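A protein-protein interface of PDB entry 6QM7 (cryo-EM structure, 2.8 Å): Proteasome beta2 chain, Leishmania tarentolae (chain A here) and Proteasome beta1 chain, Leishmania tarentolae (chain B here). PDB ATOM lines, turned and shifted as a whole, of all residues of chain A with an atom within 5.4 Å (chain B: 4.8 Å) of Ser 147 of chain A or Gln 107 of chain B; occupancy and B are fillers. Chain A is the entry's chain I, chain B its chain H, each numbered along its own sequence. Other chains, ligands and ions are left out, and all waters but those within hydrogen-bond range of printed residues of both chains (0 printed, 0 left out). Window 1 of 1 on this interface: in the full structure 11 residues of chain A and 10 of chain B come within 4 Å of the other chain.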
ATOM      1  N   LYS A 113      34.313  13.616  -0.435  1.00  0.00           N
ATOM      2  CA  LYS A 113      33.236  13.420  -1.441  1.00  0.00           C
ATOM      3  C   LYS A 113      33.700  13.856  -2.824  1.00  0.00           C
ATOM      4  O   LYS A 113      33.534  13.060  -3.769  1.00  0.00           O
ATOM      5  CB  LYS A 113      32.020  14.307  -1.170  1.00  0.00           C
ATOM      6  CG  LYS A 113      30.930  13.656  -0.345  1.00  0.00           C
ATOM      7  CD  LYS A 113      29.688  14.501  -0.264  1.00  0.00           C
ATOM      8  CE  LYS A 113      28.845  14.412  -1.513  1.00  0.00           C
ATOM      9  NZ  LYS A 113      27.426  14.714  -1.208  1.00  0.00           N
ATOM     10  N   THR A 141      29.642   8.292   6.577  1.00  0.00           N
ATOM     11  CA  THR A 141      30.394   7.423   5.652  1.00  0.00           C
ATOM     12  C   THR A 141      30.671   8.220   4.389  1.00  0.00           C
ATOM     13  O   THR A 141      29.839   9.053   4.046  1.00  0.00           O
ATOM     14  CB  THR A 141      29.597   6.193   5.220  1.00  0.00           C
ATOM     15  OG1 THR A 141      28.460   6.671   4.493  1.00  0.00           O
ATOM     16  CG2 THR A 141      29.159   5.330   6.384  1.00  0.00           C
ATOM     17  N   ILE A 142      31.793   7.965   3.736  1.00  0.00           N
ATOM     18  CA  ILE A 142      31.983   8.314   2.310  1.00  0.00           C
ATOM     19  C   ILE A 142      32.241   6.997   1.590  1.00  0.00           C
ATOM     20  O   ILE A 142      33.228   6.339   1.908  1.00  0.00           O
ATOM     21  CB  ILE A 142      33.101   9.352   2.081  1.00  0.00           C
ATOM     22  CG1 ILE A 142      33.001  10.554   3.024  1.00  0.00           C
ATOM     23  CG2 ILE A 142      33.083   9.815   0.631  1.00  0.00           C
ATOM     24  CD1 ILE A 142      33.398  10.287   4.462  1.00  0.00           C
ATOM     25  N   ALA A 143      31.350   6.629   0.677  1.00  0.00           N
ATOM     26  CA  ALA A 143      31.518   5.477  -0.232  1.00  0.00           C
ATOM     27  C   ALA A 143      32.579   5.832  -1.257  1.00  0.00           C
ATOM     28  O   ALA A 143      32.764   7.001  -1.559  1.00  0.00           O
ATOM     29  CB  ALA A 143      30.223   5.130  -0.918  1.00  0.00           C
ATOM     30  N   HIS A 145      32.616   5.854  -4.485  1.00  0.00           N
ATOM     31  CA  HIS A 145      32.041   6.642  -5.599  1.00  0.00           C
ATOM     32  C   HIS A 145      31.733   8.069  -5.154  1.00  0.00           C
ATOM     33  O   HIS A 145      31.385   8.851  -6.037  1.00  0.00           O
ATOM     34  CB  HIS A 145      30.797   5.950  -6.161  1.00  0.00           C
ATOM     35  CG  HIS A 145      31.125   4.737  -6.954  1.00  0.00           C
ATOM     36  ND1 HIS A 145      31.222   3.488  -6.368  1.00  0.00           N
ATOM     37  CD2 HIS A 145      31.417   4.582  -8.263  1.00  0.00           C
ATOM     38  CE1 HIS A 145      31.557   2.605  -7.290  1.00  0.00           C
ATOM     39  NE2 HIS A 145      31.682   3.254  -8.465  1.00  0.00           N
ATOM     40  N   GLY A 146      31.833   8.389  -3.866  1.00  0.00           N
ATOM     41  CA  GLY A 146      31.711   9.770  -3.361  1.00  0.00           C
ATOM     42  C   GLY A 146      30.307  10.103  -2.900  1.00  0.00           C
ATOM     43  O   GLY A 146      29.952  11.292  -2.864  1.00  0.00           O
ATOM     44  N   SER A 147      29.523   9.070  -2.614  1.00  0.00           N
ATOM     45  CA  SER A 147      28.245   9.138  -1.875  1.00  0.00           C
ATOM     46  C   SER A 147      28.590   9.483  -0.432  1.00  0.00           C
ATOM     47  O   SER A 147      29.653   9.067   0.017  1.00  0.00           O
ATOM     48  CB  SER A 147      27.530   7.801  -1.978  1.00  0.00           C
ATOM     49  OG  SER A 147      26.280   7.816  -1.300  1.00  0.00           O
ATOM     50  N   THR A 148      27.733  10.224   0.258  1.00  0.00           N
ATOM     51  CA  THR A 148      27.757  10.340   1.731  1.00  0.00           C
ATOM     52  C   THR A 148      26.411   9.980   2.322  1.00  0.00           C
ATOM     53  O   THR A 148      25.372  10.231   1.671  1.00  0.00           O
ATOM     54  CB  THR A 148      28.058  11.745   2.247  1.00  0.00           C
ATOM     55  OG1 THR A 148      27.238  12.711   1.584  1.00  0.00           O
ATOM     56  CG2 THR A 148      29.527  12.045   2.085  1.00  0.00           C
ATOM     57  N   ASP A 149      26.484   9.467   3.543  1.00  0.00           N
ATOM     58  CA  ASP A 149      25.344   9.269   4.455  1.00  0.00           C
ATOM     59  C   ASP A 149      25.818   9.805   5.804  1.00  0.00           C
ATOM     60  O   ASP A 149      26.785   9.250   6.332  1.00  0.00           O
ATOM     61  CB  ASP A 149      24.917   7.794   4.432  1.00  0.00           C
ATOM     62  CG  ASP A 149      24.333   7.305   3.101  1.00  0.00           C
ATOM     63  OD1 ASP A 149      23.315   7.896   2.638  1.00  0.00           O
ATOM     64  OD2 ASP A 149      24.880   6.315   2.538  1.00  0.00           O
ATOM     65  N   ARG B  99      15.985  12.416  -5.636  1.00  0.00           N
ATOM     66  CA  ARG B  99      17.158  11.767  -6.248  1.00  0.00           C
ATOM     67  C   ARG B  99      16.897  10.264  -6.290  1.00  0.00           C
ATOM     68  O   ARG B  99      16.638   9.652  -5.225  1.00  0.00           O
ATOM     69  CB  ARG B  99      18.399  12.109  -5.426  1.00  0.00           C
ATOM     70  CG  ARG B  99      18.709  13.598  -5.312  1.00  0.00           C
ATOM     71  CD  ARG B  99      19.980  13.827  -4.509  1.00  0.00           C
ATOM     72  NE  ARG B  99      19.843  13.438  -3.112  1.00  0.00           N
ATOM     73  CZ  ARG B  99      20.266  12.299  -2.566  1.00  0.00           C
ATOM     74  NH1 ARG B  99      20.077  12.082  -1.277  1.00  0.00           N
ATOM     75  NH2 ARG B  99      20.890  11.373  -3.275  1.00  0.00           N
ATOM     76  N   ALA B 103      23.535   7.300  -5.793  1.00  0.00           N
ATOM     77  CA  ALA B 103      23.519   8.301  -4.709  1.00  0.00           C
ATOM     78  C   ALA B 103      24.670   9.276  -4.938  1.00  0.00           C
ATOM     79  O   ALA B 103      24.436  10.486  -4.847  1.00  0.00           O
ATOM     80  CB  ALA B 103      23.614   7.627  -3.360  1.00  0.00           C
ATOM     81  N   ALA B 104      25.853   8.754  -5.249  1.00  0.00           N
ATOM     82  CA  ALA B 104      27.058   9.529  -5.614  1.00  0.00           C
ATOM     83  C   ALA B 104      26.728  10.573  -6.685  1.00  0.00           C
ATOM     84  O   ALA B 104      27.059  11.746  -6.482  1.00  0.00           O
ATOM     85  CB  ALA B 104      28.121   8.581  -6.101  1.00  0.00           C
ATOM     86  N   ASP B 105      26.085  10.139  -7.769  1.00  0.00           N
ATOM     87  CA  ASP B 105      25.856  10.939  -8.997  1.00  0.00           C
ATOM     88  C   ASP B 105      24.818  12.024  -8.720  1.00  0.00           C
ATOM     89  O   ASP B 105      25.024  13.156  -9.148  1.00  0.00           O
ATOM     90  CB  ASP B 105      25.452  10.046 -10.171  1.00  0.00           C
ATOM     91  CG  ASP B 105      26.572   9.147 -10.696  1.00  0.00           C
ATOM     92  OD1 ASP B 105      27.760   9.578 -10.668  1.00  0.00           O
ATOM     93  OD2 ASP B 105      26.259   8.014 -11.150  1.00  0.00           O
ATOM     94  N   THR B 106      23.735  11.689  -8.038  1.00  0.00           N
ATOM     95  CA  THR B 106      22.636  12.643  -7.761  1.00  0.00           C
ATOM     96  C   THR B 106      23.061  13.653  -6.696  1.00  0.00           C
ATOM     97  O   THR B 106      22.640  14.816  -6.811  1.00  0.00           O
ATOM     98  CB  THR B 106      21.370  11.913  -7.323  1.00  0.00           C
ATOM     99  OG1 THR B 106      21.656  11.155  -6.148  1.00  0.00           O
ATOM    100  CG2 THR B 106      20.856  11.023  -8.428  1.00  0.00           C
ATOM    101  N   GLN B 107      23.802  13.216  -5.677  1.00  0.00           N
ATOM    102  CA  GLN B 107      24.326  14.108  -4.617  1.00  0.00           C
ATOM    103  C   GLN B 107      25.253  15.144  -5.260  1.00  0.00           C
ATOM    104  O   GLN B 107      25.166  16.329  -4.896  1.00  0.00           O
ATOM    105  CB  GLN B 107      25.102  13.313  -3.571  1.00  0.00           C
ATOM    106  CG  GLN B 107      24.224  12.626  -2.543  1.00  0.00           C
ATOM    107  CD  GLN B 107      25.058  11.852  -1.556  1.00  0.00           C
ATOM    108  OE1 GLN B 107      26.232  12.148  -1.352  1.00  0.00           O
ATOM    109  NE2 GLN B 107      24.461  10.851  -0.925  1.00  0.00           N
ATOM    110  N   ALA B 108      26.110  14.686  -6.177  1.00  0.00           N
ATOM    111  CA  ALA B 108      27.109  15.493  -6.899  1.00  0.00           C
ATOM    112  C   ALA B 108      26.406  16.532  -7.762  1.00  0.00           C
ATOM    113  O   ALA B 108      26.841  17.691  -7.755  1.00  0.00           O
ATOM    114  CB  ALA B 108      27.965  14.603  -7.745  1.00  0.00           C
ATOM    115  N   LEU B 109      25.388  16.114  -8.507  1.00  0.00           N
ATOM    116  CA  LEU B 109      24.556  17.013  -9.334  1.00  0.00           C
ATOM    117  C   LEU B 109      23.777  17.959  -8.435  1.00  0.00           C
ATOM    118  O   LEU B 109      23.813  19.159  -8.703  1.00  0.00           O
ATOM    119  CB  LEU B 109      23.598  16.185 -10.182  1.00  0.00           C
ATOM    120  CG  LEU B 109      24.252  15.401 -11.319  1.00  0.00           C
ATOM    121  CD1 LEU B 109      23.261  14.406 -11.909  1.00  0.00           C
ATOM    122  CD2 LEU B 109      24.773  16.347 -12.393  1.00  0.00           C
ATOM    123  N   ALA B 110      23.101  17.449  -7.415  1.00  0.00           N
ATOM    124  CA  ALA B 110      22.260  18.276  -6.526  1.00  0.00           C
ATOM    125  C   ALA B 110      23.115  19.360  -5.868  1.00  0.00           C
ATOM    126  O   ALA B 110      22.598  20.482  -5.717  1.00  0.00           O
ATOM    127  CB  ALA B 110      21.548  17.430  -5.506  1.00  0.00           C
ATOM    128  N   GLU B 111      24.368  19.054  -5.524  1.00  0.00           N
ATOM    129  CA  GLU B 111      25.282  20.017  -4.856  1.00  0.00           C
ATOM    130  C   GLU B 111      25.782  21.029  -5.877  1.00  0.00           C
ATOM    131  O   GLU B 111      25.939  22.204  -5.507  1.00  0.00           O
ATOM    132  CB  GLU B 111      26.463  19.316  -4.188  1.00  0.00           C
ATOM    133  CG  GLU B 111      26.130  18.787  -2.797  1.00  0.00           C
ATOM    134  CD  GLU B 111      27.120  17.774  -2.230  1.00  0.00           C
ATOM    135  OE1 GLU B 111      27.455  16.802  -2.957  1.00  0.00           O
ATOM    136  OE2 GLU B 111      27.570  17.957  -1.067  1.00  0.00           O
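The side-chain amide nitrogen (NE2) of Gln 107 of chain B is in hydrogen-bond range of the backbone carbonyl oxygen (O) of Thr 148 of chain A. The side-chain amide oxygen (OE1) of Gln 107 of chain B sits at hydrogen-bond distance from the side-chain amino group (NZ) of Lys 113 of chain A, at 2.8 Å. The side-chain amino group of Lys 113 of chain A is in salt-bridge range of the side-chain carboxylate of Glu 111 of chain B, 2.7 Å away.
The backbone carbonyl oxygen of Ala 103 of chain B is in hydrogen-bond range of the side-chain hydroxyl of Thr 106 of chain B (3.1 Å). NZ of Lys 113 of chain A sits at hydrogen-bond distance from OG1 of Thr 148 of chain A (3.4 Å).
Among the printed residues, merely in contact across the chains: His 145 of chain A with Ala 104 of chain B (3.3 Å), Ser 147 of chain A with Ala 103 of chain B (3.4 Å), Ser 147 of chain A with Gln 107 of chain B (3.6 Å) and Ser 147 of chain A with Ala 104 of chain B (3.8 Å).
Ser 147 of chain A touches just these residues of chain B: Ala 103, Ala 104 and Gln 107. Of chain A, only Lys 113, Ser 147 and Thr 148 come within 4 Å of Gln 107 of chain B. Of the printed residues of chain A, Ala 104 of chain B touches His 145 (3.3 Å) and Ser 147 (3.8 Å). Of the printed residues of chain B, Thr 148 of chain A touches Gln 107. The nearest residue of chain A that does not touch Gln 107 of chain B is Gly 146 of chain A (4.1 Å). The nearest printed residue of chain A that does not touch Glu 111 of chain B is Thr 148 of chain A (5.9 Å).
Of the 9 printed residues of chain A, 4 touch a printed residue of chain B. Hydrophobic or aromatic side chains of chain A within 4 Å of the printed part of chain B: His 145. Among the printed residues, 7 pairs touch across the chains.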
